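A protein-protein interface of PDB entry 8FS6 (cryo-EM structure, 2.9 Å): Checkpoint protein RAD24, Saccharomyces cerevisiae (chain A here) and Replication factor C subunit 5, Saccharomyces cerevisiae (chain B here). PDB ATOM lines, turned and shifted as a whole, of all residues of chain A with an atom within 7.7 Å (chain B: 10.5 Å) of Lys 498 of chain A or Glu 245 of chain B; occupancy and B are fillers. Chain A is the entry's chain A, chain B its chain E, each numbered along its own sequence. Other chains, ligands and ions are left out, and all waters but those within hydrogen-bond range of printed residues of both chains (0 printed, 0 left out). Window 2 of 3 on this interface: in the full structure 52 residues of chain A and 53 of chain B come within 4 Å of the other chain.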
ATOM      1  N   LEU A 490      15.709  21.322 -13.196  1.00  0.00           N
ATOM      2  CA  LEU A 490      16.164  19.983 -12.834  1.00  0.00           C
ATOM      3  C   LEU A 490      15.272  19.366 -11.763  1.00  0.00           C
ATOM      4  O   LEU A 490      14.942  18.175 -11.826  1.00  0.00           O
ATOM      5  CB  LEU A 490      17.618  20.027 -12.361  1.00  0.00           C
ATOM      6  CG  LEU A 490      18.685  19.672 -13.400  1.00  0.00           C
ATOM      7  CD1 LEU A 490      18.877  20.804 -14.394  1.00  0.00           C
ATOM      8  CD2 LEU A 490      19.999  19.320 -12.719  1.00  0.00           C
ATOM      9  N   ILE A 491      14.871  20.166 -10.772  1.00  0.00           N
ATOM     10  CA  ILE A 491      14.013  19.657  -9.705  1.00  0.00           C
ATOM     11  C   ILE A 491      12.660  19.234 -10.265  1.00  0.00           C
ATOM     12  O   ILE A 491      12.147  18.157  -9.938  1.00  0.00           O
ATOM     13  CB  ILE A 491      13.873  20.710  -8.590  1.00  0.00           C
ATOM     14  CG1 ILE A 491      15.198  20.848  -7.837  1.00  0.00           C
ATOM     15  CG2 ILE A 491      12.748  20.340  -7.635  1.00  0.00           C
ATOM     16  CD1 ILE A 491      15.167  21.854  -6.713  1.00  0.00           C
ATOM     17  N   ARG A 492      12.071  20.058 -11.133  1.00  0.00           N
ATOM     18  CA  ARG A 492      10.818  19.694 -11.783  1.00  0.00           C
ATOM     19  C   ARG A 492      10.978  18.549 -12.774  1.00  0.00           C
ATOM     20  O   ARG A 492       9.982  17.901 -13.113  1.00  0.00           O
ATOM     21  CB  ARG A 492      10.214  20.912 -12.489  1.00  0.00           C
ATOM     22  CG  ARG A 492       9.861  22.061 -11.554  1.00  0.00           C
ATOM     23  CD  ARG A 492       9.216  21.558 -10.270  1.00  0.00           C
ATOM     24  NE  ARG A 492       8.632  22.641  -9.486  1.00  0.00           N
ATOM     25  CZ  ARG A 492       8.129  22.494  -8.268  1.00  0.00           C
ATOM     26  NH1 ARG A 492       8.126  21.320  -7.657  1.00  0.00           N
ATOM     27  NH2 ARG A 492       7.617  23.552  -7.647  1.00  0.00           N
ATOM     28  N   LYS A 493      12.208  18.279 -13.213  1.00  0.00           N
ATOM     29  CA  LYS A 493      12.427  17.122 -14.122  1.00  0.00           C
ATOM     30  C   LYS A 493      12.523  15.838 -13.292  1.00  0.00           C
ATOM     31  O   LYS A 493      12.174  14.767 -13.824  1.00  0.00           O
ATOM     32  CB  LYS A 493      13.681  17.330 -14.976  1.00  0.00           C
ATOM     33  CG  LYS A 493      13.661  16.613 -16.319  1.00  0.00           C
ATOM     34  CD  LYS A 493      12.429  16.947 -17.131  1.00  0.00           C
ATOM     35  CE  LYS A 493      12.316  16.145 -18.409  1.00  0.00           C
ATOM     36  NZ  LYS A 493      11.103  16.512 -19.177  1.00  0.00           N
ATOM     37  N   CYS A 494      12.968  15.948 -12.037  1.00  0.00           N
ATOM     38  CA  CYS A 494      13.151  14.747 -11.179  1.00  0.00           C
ATOM     39  C   CYS A 494      11.960  14.597 -10.227  1.00  0.00           C
ATOM     40  O   CYS A 494      11.367  13.505 -10.187  1.00  0.00           O
ATOM     41  CB  CYS A 494      14.437  14.857 -10.370  1.00  0.00           C
ATOM     42  SG  CYS A 494      15.909  15.127 -11.392  1.00  0.00           S
ATOM     43  N   GLN A 495      11.627  15.658  -9.490  1.00  0.00           N
ATOM     44  CA  GLN A 495      10.522  15.584  -8.496  1.00  0.00           C
ATOM     45  C   GLN A 495       9.210  15.251  -9.212  1.00  0.00           C
ATOM     46  O   GLN A 495       8.451  14.415  -8.682  1.00  0.00           O
ATOM     47  CB  GLN A 495      10.397  16.908  -7.742  1.00  0.00           C
ATOM     48  CG  GLN A 495       9.274  16.926  -6.716  1.00  0.00           C
ATOM     49  CD  GLN A 495       9.036  18.307  -6.159  1.00  0.00           C
ATOM     50  OE1 GLN A 495       9.693  19.274  -6.539  1.00  0.00           O
ATOM     51  NE2 GLN A 495       8.084  18.410  -5.247  1.00  0.00           N
ATOM     52  N   SER A 496       8.958  15.865 -10.370  1.00  0.00           N
ATOM     53  CA  SER A 496       7.655  15.663 -11.055  1.00  0.00           C
ATOM     54  C   SER A 496       7.773  14.636 -12.185  1.00  0.00           C
ATOM     55  O   SER A 496       7.085  13.601 -12.108  1.00  0.00           O
ATOM     56  CB  SER A 496       7.116  16.973 -11.571  1.00  0.00           C
ATOM     57  OG  SER A 496       5.882  16.782 -12.244  1.00  0.00           O
ATOM     58  N   TYR A 497       8.611  14.905 -13.189  1.00  0.00           N
ATOM     59  CA  TYR A 497       8.685  14.002 -14.370  1.00  0.00           C
ATOM     60  C   TYR A 497       9.151  12.600 -13.963  1.00  0.00           C
ATOM     61  O   TYR A 497       8.470  11.625 -14.335  1.00  0.00           O
ATOM     62  CB  TYR A 497       9.606  14.595 -15.438  1.00  0.00           C
ATOM     63  CG  TYR A 497      10.043  13.619 -16.501  1.00  0.00           C
ATOM     64  CD1 TYR A 497       9.126  13.042 -17.363  1.00  0.00           C
ATOM     65  CD2 TYR A 497      11.374  13.256 -16.633  1.00  0.00           C
ATOM     66  CE1 TYR A 497       9.519  12.141 -18.337  1.00  0.00           C
ATOM     67  CE2 TYR A 497      11.784  12.356 -17.601  1.00  0.00           C
ATOM     68  CZ  TYR A 497      10.853  11.796 -18.458  1.00  0.00           C
ATOM     69  OH  TYR A 497      11.252  10.901 -19.421  1.00  0.00           O
ATOM     70  N   LYS A 498      10.262  12.493 -13.229  1.00  0.00           N
ATOM     71  CA  LYS A 498      10.812  11.148 -12.904  1.00  0.00           C
ATOM     72  C   LYS A 498       9.800  10.354 -12.068  1.00  0.00           C
ATOM     73  O   LYS A 498       9.640   9.149 -12.334  1.00  0.00           O
ATOM     74  CB  LYS A 498      12.162  11.263 -12.189  1.00  0.00           C
ATOM     75  CG  LYS A 498      13.357  11.515 -13.098  1.00  0.00           C
ATOM     76  CD  LYS A 498      14.660  11.653 -12.341  1.00  0.00           C
ATOM     77  CE  LYS A 498      14.899  10.527 -11.358  1.00  0.00           C
ATOM     78  NZ  LYS A 498      14.988   9.213 -12.037  1.00  0.00           N
ATOM     79  N   LYS A 499       9.148  11.005 -11.102  1.00  0.00           N
ATOM     80  CA  LYS A 499       8.169  10.307 -10.225  1.00  0.00           C
ATOM     81  C   LYS A 499       6.773  10.899 -10.445  1.00  0.00           C
ATOM     82  O   LYS A 499       6.179  10.581 -11.494  1.00  0.00           O
ATOM     83  CB  LYS A 499       8.589  10.421  -8.757  1.00  0.00           C
ATOM     84  CG  LYS A 499       7.677   9.712  -7.766  1.00  0.00           C
ATOM     85  CD  LYS A 499       8.147   9.830  -6.333  1.00  0.00           C
ATOM     86  CE  LYS A 499       7.240   9.116  -5.353  1.00  0.00           C
ATOM     87  NZ  LYS A 499       7.718   9.260  -3.957  1.00  0.00           N
ATOM     88  N   TRP B   4      12.182  23.366  -1.504  1.00  0.00           N
ATOM     89  CA  TRP B   4      12.548  23.334  -0.093  1.00  0.00           C
ATOM     90  C   TRP B   4      12.987  24.694   0.430  1.00  0.00           C
ATOM     91  O   TRP B   4      13.042  24.880   1.650  1.00  0.00           O
ATOM     92  CB  TRP B   4      13.653  22.303   0.146  1.00  0.00           C
ATOM     93  CG  TRP B   4      13.259  20.893  -0.201  1.00  0.00           C
ATOM     94  CD1 TRP B   4      12.021  20.453  -0.577  1.00  0.00           C
ATOM     95  CD2 TRP B   4      14.106  19.737  -0.191  1.00  0.00           C
ATOM     96  NE1 TRP B   4      12.048  19.101  -0.810  1.00  0.00           N
ATOM     97  CE2 TRP B   4      13.316  18.637  -0.578  1.00  0.00           C
ATOM     98  CE3 TRP B   4      15.456  19.526   0.105  1.00  0.00           C
ATOM     99  CZ2 TRP B   4      13.831  17.345  -0.678  1.00  0.00           C
ATOM    100  CZ3 TRP B   4      15.965  18.243   0.008  1.00  0.00           C
ATOM    101  CH2 TRP B   4      15.154  17.170  -0.382  1.00  0.00           C
ATOM    102  N   GLU B 209      12.583  16.164   6.037  1.00  0.00           N
ATOM    103  CA  GLU B 209      12.221  15.519   4.780  1.00  0.00           C
ATOM    104  C   GLU B 209      12.477  14.016   4.788  1.00  0.00           C
ATOM    105  O   GLU B 209      12.111  13.338   3.820  1.00  0.00           O
ATOM    106  CB  GLU B 209      12.979  16.173   3.618  1.00  0.00           C
ATOM    107  CG  GLU B 209      12.311  16.036   2.247  1.00  0.00           C
ATOM    108  CD  GLU B 209      11.176  17.023   2.013  1.00  0.00           C
ATOM    109  OE1 GLU B 209      10.581  17.519   2.994  1.00  0.00           O
ATOM    110  OE2 GLU B 209      10.874  17.303   0.835  1.00  0.00           O
ATOM    111  N   ARG B 210      13.099  13.490   5.843  1.00  0.00           N
ATOM    112  CA  ARG B 210      13.349  12.066   6.060  1.00  0.00           C
ATOM    113  C   ARG B 210      14.277  11.450   5.022  1.00  0.00           C
ATOM    114  O   ARG B 210      14.303  10.220   4.885  1.00  0.00           O
ATOM    115  CB  ARG B 210      12.049  11.255   6.108  1.00  0.00           C
ATOM    116  CG  ARG B 210      11.324  11.301   7.441  1.00  0.00           C
ATOM    117  CD  ARG B 210       9.830  11.487   7.237  1.00  0.00           C
ATOM    118  NE  ARG B 210       9.419  11.126   5.885  1.00  0.00           N
ATOM    119  CZ  ARG B 210       8.421  11.698   5.226  1.00  0.00           C
ATOM    120  NH1 ARG B 210       7.700  12.666   5.769  1.00  0.00           N
ATOM    121  NH2 ARG B 210       8.139  11.289   3.993  1.00  0.00           N
ATOM    122  N   ILE B 211      15.034  12.258   4.278  1.00  0.00           N
ATOM    123  CA  ILE B 211      16.012  11.700   3.355  1.00  0.00           C
ATOM    124  C   ILE B 211      17.149  11.076   4.154  1.00  0.00           C
ATOM    125  O   ILE B 211      17.492  11.535   5.254  1.00  0.00           O
ATOM    126  CB  ILE B 211      16.511  12.774   2.369  1.00  0.00           C
ATOM    127  CG1 ILE B 211      17.723  13.532   2.919  1.00  0.00           C
ATOM    128  CG2 ILE B 211      15.388  13.742   2.023  1.00  0.00           C
ATOM    129  CD1 ILE B 211      18.377  14.448   1.907  1.00  0.00           C
ATOM    130  N   GLN B 212      17.710   9.991   3.627  1.00  0.00           N
ATOM    131  CA  GLN B 212      18.740   9.236   4.336  1.00  0.00           C
ATOM    132  C   GLN B 212      20.105   9.728   3.877  1.00  0.00           C
ATOM    133  O   GLN B 212      20.547   9.429   2.765  1.00  0.00           O
ATOM    134  CB  GLN B 212      18.584   7.739   4.095  1.00  0.00           C
ATOM    135  CG  GLN B 212      19.685   6.905   4.737  1.00  0.00           C
ATOM    136  CD  GLN B 212      19.680   5.465   4.266  1.00  0.00           C
ATOM    137  OE1 GLN B 212      18.792   5.046   3.526  1.00  0.00           O
ATOM    138  NE2 GLN B 212      20.677   4.700   4.694  1.00  0.00           N
ATOM    139  N   LEU B 213      20.778  10.482   4.737  1.00  0.00           N
ATOM    140  CA  LEU B 213      22.138  10.912   4.465  1.00  0.00           C
ATOM    141  C   LEU B 213      23.110  10.032   5.236  1.00  0.00           C
ATOM    142  O   LEU B 213      22.762   9.451   6.269  1.00  0.00           O
ATOM    143  CB  LEU B 213      22.340  12.381   4.845  1.00  0.00           C
ATOM    144  CG  LEU B 213      22.702  12.706   6.297  1.00  0.00           C
ATOM    145  CD1 LEU B 213      24.195  12.893   6.442  1.00  0.00           C
ATOM    146  CD2 LEU B 213      21.988  13.944   6.759  1.00  0.00           C
ATOM    147  N   LEU B 237      21.059  20.914  -2.207  1.00  0.00           N
ATOM    148  CA  LEU B 237      20.658  19.751  -1.423  1.00  0.00           C
ATOM    149  C   LEU B 237      19.477  19.041  -2.067  1.00  0.00           C
ATOM    150  O   LEU B 237      19.463  17.809  -2.174  1.00  0.00           O
ATOM    151  CB  LEU B 237      20.316  20.177   0.006  1.00  0.00           C
ATOM    152  CG  LEU B 237      19.786  19.068   0.916  1.00  0.00           C
ATOM    153  CD1 LEU B 237      20.835  17.984   1.106  1.00  0.00           C
ATOM    154  CD2 LEU B 237      19.337  19.626   2.256  1.00  0.00           C
ATOM    155  N   GLU B 238      18.476  19.805  -2.514  1.00  0.00           N
ATOM    156  CA  GLU B 238      17.314  19.193  -3.149  1.00  0.00           C
ATOM    157  C   GLU B 238      17.694  18.503  -4.454  1.00  0.00           C
ATOM    158  O   GLU B 238      17.244  17.382  -4.721  1.00  0.00           O
ATOM    159  CB  GLU B 238      16.228  20.241  -3.390  1.00  0.00           C
ATOM    160  CG  GLU B 238      14.866  19.644  -3.715  1.00  0.00           C
ATOM    161  CD  GLU B 238      13.752  20.671  -3.681  1.00  0.00           C
ATOM    162  OE1 GLU B 238      14.053  21.872  -3.519  1.00  0.00           O
ATOM    163  OE2 GLU B 238      12.575  20.278  -3.819  1.00  0.00           O
ATOM    164  N   SER B 239      18.528  19.150  -5.274  1.00  0.00           N
ATOM    165  CA  SER B 239      18.947  18.544  -6.533  1.00  0.00           C
ATOM    166  C   SER B 239      19.753  17.273  -6.298  1.00  0.00           C
ATOM    167  O   SER B 239      19.557  16.268  -6.992  1.00  0.00           O
ATOM    168  CB  SER B 239      19.755  19.548  -7.356  1.00  0.00           C
ATOM    169  OG  SER B 239      19.057  20.776  -7.489  1.00  0.00           O
ATOM    170  N   MET B 240      20.665  17.295  -5.322  1.00  0.00           N
ATOM    171  CA  MET B 240      21.477  16.118  -5.036  1.00  0.00           C
ATOM    172  C   MET B 240      20.631  14.979  -4.480  1.00  0.00           C
ATOM    173  O   MET B 240      20.837  13.815  -4.841  1.00  0.00           O
ATOM    174  CB  MET B 240      22.599  16.480  -4.064  1.00  0.00           C
ATOM    175  CG  MET B 240      23.835  17.056  -4.736  1.00  0.00           C
ATOM    176  SD  MET B 240      24.912  17.931  -3.586  1.00  0.00           S
ATOM    177  CE  MET B 240      25.158  16.674  -2.333  1.00  0.00           C
ATOM    178  N   ALA B 241      19.679  15.292  -3.595  1.00  0.00           N
ATOM    179  CA  ALA B 241      18.809  14.256  -3.049  1.00  0.00           C
ATOM    180  C   ALA B 241      17.918  13.652  -4.127  1.00  0.00           C
ATOM    181  O   ALA B 241      17.703  12.435  -4.150  1.00  0.00           O
ATOM    182  CB  ALA B 241      17.964  14.826  -1.910  1.00  0.00           C
ATOM    183  N   LEU B 242      17.389  14.486  -5.027  1.00  0.00           N
ATOM    184  CA  LEU B 242      16.523  13.974  -6.084  1.00  0.00           C
ATOM    185  C   LEU B 242      17.304  13.167  -7.113  1.00  0.00           C
ATOM    186  O   LEU B 242      16.803  12.153  -7.612  1.00  0.00           O
ATOM    187  CB  LEU B 242      15.785  15.129  -6.760  1.00  0.00           C
ATOM    188  CG  LEU B 242      14.371  15.462  -6.276  1.00  0.00           C
ATOM    189  CD1 LEU B 242      14.252  15.375  -4.759  1.00  0.00           C
ATOM    190  CD2 LEU B 242      13.971  16.844  -6.761  1.00  0.00           C
ATOM    191  N   ASN B 243      18.523  13.597  -7.445  1.00  0.00           N
ATOM    192  CA  ASN B 243      19.340  12.870  -8.409  1.00  0.00           C
ATOM    193  C   ASN B 243      19.939  11.596  -7.831  1.00  0.00           C
ATOM    194  O   ASN B 243      20.277  10.685  -8.595  1.00  0.00           O
ATOM    195  CB  ASN B 243      20.456  13.773  -8.937  1.00  0.00           C
ATOM    196  CG  ASN B 243      19.991  14.681 -10.058  1.00  0.00           C
ATOM    197  OD1 ASN B 243      19.003  15.402  -9.918  1.00  0.00           O
ATOM    198  ND2 ASN B 243      20.702  14.651 -11.178  1.00  0.00           N
ATOM    199  N   ASN B 244      20.081  11.510  -6.509  1.00  0.00           N
ATOM    200  CA  ASN B 244      20.603  10.320  -5.850  1.00  0.00           C
ATOM    201  C   ASN B 244      19.508   9.500  -5.179  1.00  0.00           C
ATOM    202  O   ASN B 244      19.819   8.592  -4.400  1.00  0.00           O
ATOM    203  CB  ASN B 244      21.674  10.706  -4.827  1.00  0.00           C
ATOM    204  CG  ASN B 244      23.035  10.927  -5.460  1.00  0.00           C
ATOM    205  OD1 ASN B 244      24.064  10.842  -4.789  1.00  0.00           O
ATOM    206  ND2 ASN B 244      23.049  11.211  -6.757  1.00  0.00           N
ATOM    207  N   GLU B 245      18.240   9.806  -5.461  1.00  0.00           N
ATOM    208  CA  GLU B 245      17.083   9.085  -4.927  1.00  0.00           C
ATOM    209  C   GLU B 245      17.064   9.118  -3.395  1.00  0.00           C
ATOM    210  O   GLU B 245      17.007   8.086  -2.722  1.00  0.00           O
ATOM    211  CB  GLU B 245      17.037   7.646  -5.454  1.00  0.00           C
ATOM    212  CG  GLU B 245      17.246   7.525  -6.957  1.00  0.00           C
ATOM    213  CD  GLU B 245      16.274   8.372  -7.757  1.00  0.00           C
ATOM    214  OE1 GLU B 245      15.075   8.405  -7.404  1.00  0.00           O
ATOM    215  OE2 GLU B 245      16.708   9.007  -8.740  1.00  0.00           O
ATOM    216  N   LEU B 246      17.110  10.341  -2.861  1.00  0.00           N
ATOM    217  CA  LEU B 246      16.971  10.600  -1.424  1.00  0.00           C
ATOM    218  C   LEU B 246      18.027   9.852  -0.611  1.00  0.00           C
ATOM    219  O   LEU B 246      17.754   9.345   0.479  1.00  0.00           O
ATOM    220  CB  LEU B 246      15.563  10.254  -0.923  1.00  0.00           C
ATOM    221  CG  LEU B 246      14.305  11.079  -1.253  1.00  0.00           C
ATOM    222  CD1 LEU B 246      14.201  11.537  -2.707  1.00  0.00           C
ATOM    223  CD2 LEU B 246      13.055  10.304  -0.849  1.00  0.00           C
ATOM    224  N   ALA B 247      19.249   9.788  -1.141  1.00  0.00           N
ATOM    225  CA  ALA B 247      20.331   9.063  -0.475  1.00  0.00           C
ATOM    226  C   ALA B 247      21.636   9.794  -0.775  1.00  0.00           C
ATOM    227  O   ALA B 247      22.222   9.609  -1.846  1.00  0.00           O
ATOM    228  CB  ALA B 247      20.384   7.611  -0.931  1.00  0.00           C
ATOM    229  N   LEU B 248      22.087  10.612   0.174  1.00  0.00           N
ATOM    230  CA  LEU B 248      23.316  11.387   0.016  1.00  0.00           C
ATOM    231  C   LEU B 248      24.507  10.472   0.271  1.00  0.00           C
ATOM    232  O   LEU B 248      24.953  10.291   1.405  1.00  0.00           O
ATOM    233  CB  LEU B 248      23.322  12.586   0.956  1.00  0.00           C
ATOM    234  CG  LEU B 248      22.221  13.624   0.739  1.00  0.00           C
ATOM    235  CD1 LEU B 248      22.223  14.644   1.865  1.00  0.00           C
ATOM    236  CD2 LEU B 248      22.393  14.309  -0.608  1.00  0.00           C
ATOM    237  N   LYS B 249      25.023   9.879  -0.802  1.00  0.00           N
ATOM    238  CA  LYS B 249      26.227   9.070  -0.705  1.00  0.00           C
ATOM    239  C   LYS B 249      27.454   9.966  -0.563  1.00  0.00           C
ATOM    240  O   LYS B 249      27.455  11.123  -0.989  1.00  0.00           O
ATOM    241  CB  LYS B 249      26.369   8.174  -1.934  1.00  0.00           C
ATOM    242  CG  LYS B 249      25.244   7.168  -2.096  1.00  0.00           C
ATOM    243  CD  LYS B 249      24.874   6.989  -3.558  1.00  0.00           C
ATOM    244  CE  LYS B 249      23.375   6.807  -3.726  1.00  0.00           C
ATOM    245  NZ  LYS B 249      22.805   5.924  -2.671  1.00  0.00           N
ATOM    246  N   SER B 252      28.575  11.777  -3.598  1.00  0.00           N
ATOM    247  CA  SER B 252      27.528  12.477  -4.332  1.00  0.00           C
ATOM    248  C   SER B 252      28.119  13.694  -5.031  1.00  0.00           C
ATOM    249  O   SER B 252      28.809  14.495  -4.390  1.00  0.00           O
ATOM    250  CB  SER B 252      26.401  12.905  -3.394  1.00  0.00           C
ATOM    251  OG  SER B 252      25.150  12.900  -4.060  1.00  0.00           O
ATOM    252  N   PRO B 253      27.884  13.867  -6.331  1.00  0.00           N
ATOM    253  CA  PRO B 253      28.472  15.011  -7.039  1.00  0.00           C
ATOM    254  C   PRO B 253      27.814  16.315  -6.612  1.00  0.00           C
ATOM    255  O   PRO B 253      26.591  16.460  -6.670  1.00  0.00           O
ATOM    256  CB  PRO B 253      28.200  14.695  -8.514  1.00  0.00           C
ATOM    257  CG  PRO B 253      26.997  13.811  -8.493  1.00  0.00           C
ATOM    258  CD  PRO B 253      27.070  13.017  -7.217  1.00  0.00           C
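The backbone NH (N) of Trp 4 of chain B sits at hydrogen-bond distance from the side-chain carboxylate (OE1) of Glu 238 of chain B (3.1 Å).
O of Cys 494 of chain A sits at hydrogen-bond distance from N of Lys 499 of chain A (3.5 Å).
The side-chain amide oxygen (OE1) of Gln 495 of chain A lies within hydrogen-bond range of the guanidinium group (NH1) of Arg 492 of chain A, 2.8 Å away.
The side-chain sulfur of Cys 494 of chain A sits at hydrogen-bond distance from the backbone carbonyl oxygen of Leu 490 of chain A, 3.2 Å away.
OD1 of Asn 243 of chain B lies close to O of Ser 239 of chain B (3.1 Å).
N of Lys 498 of chain A sits at hydrogen-bond distance from O of Lys 493 of chain A (3.0 Å).
Hydrophobic or aromatic side chains of chain A that line the printed part of chain B: Ile 491.
Of the 21 printed residues of chain B, 5 touch a printed residue of chain A.
Hydrophobic or aromatic side chains of chain B within 4 Å of the printed part of chain A: Leu 242.
Among the printed residues, 7 pairs touch across the chains.
Among the printed residues, Asp or Glu carboxylates within 4 Å of a Lys or Arg side-chain nitrogen of the other chain: Lys 498 of chain A with Glu 245 of chain B (3.7 Å).
Of chain A, only Lys 498 comes within 4 Å of Glu 245 of chain B.
Cys 494 of chain A touches just these residues of chain B: Leu 242 and Asn 243.
No residue of chain B comes within 4 Å of Ser 496 of chain A.
Of the printed residues of chain A, Ser 239 of chain B touches Ile 491.
Printed residues of chain A within 4 Å of Leu 242 of chain B: Ile 491, Cys 494 and Gln 495.
Of the printed residues of chain A, Glu 238 of chain B touches Ile 491.
Of the printed residues of chain A, Asn 243 of chain B touches Cys 494 (3.4 Å).
Lys 249 of chain B touches none of the printed residues of chain A.
The nearest residue of chain B that does not touch Lys 498 of chain A is Leu 242 of chain B (4.5 Å).
The nearest residue of chain A that does not touch Glu 245 of chain B is Cys 494 of chain A (6.5 Å).
OE2 of Glu 245 of chain B lies within salt-bridge range of NZ of Lys 498 of chain A (3.7 Å).
The side-chain sulfur of Cys 494 of chain A sits at hydrogen-bond distance from the side-chain amide oxygen of Asn 243 of chain B, at 3.4 Å.
Among the printed residues, pairs that only touch across the chains: Ile 491 of chain A with Glu 238 of chain B (3.4 Å), Gln 495 of chain A with Leu 242 of chain B (3.7 Å), Ile 491 of chain A with Leu 242 of chain B (3.8 Å), Cys 494 of chain A with Leu 242 of chain B (3.9 Å) and Ile 491 of chain A with Ser 239 of chain B (3.9 Å).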
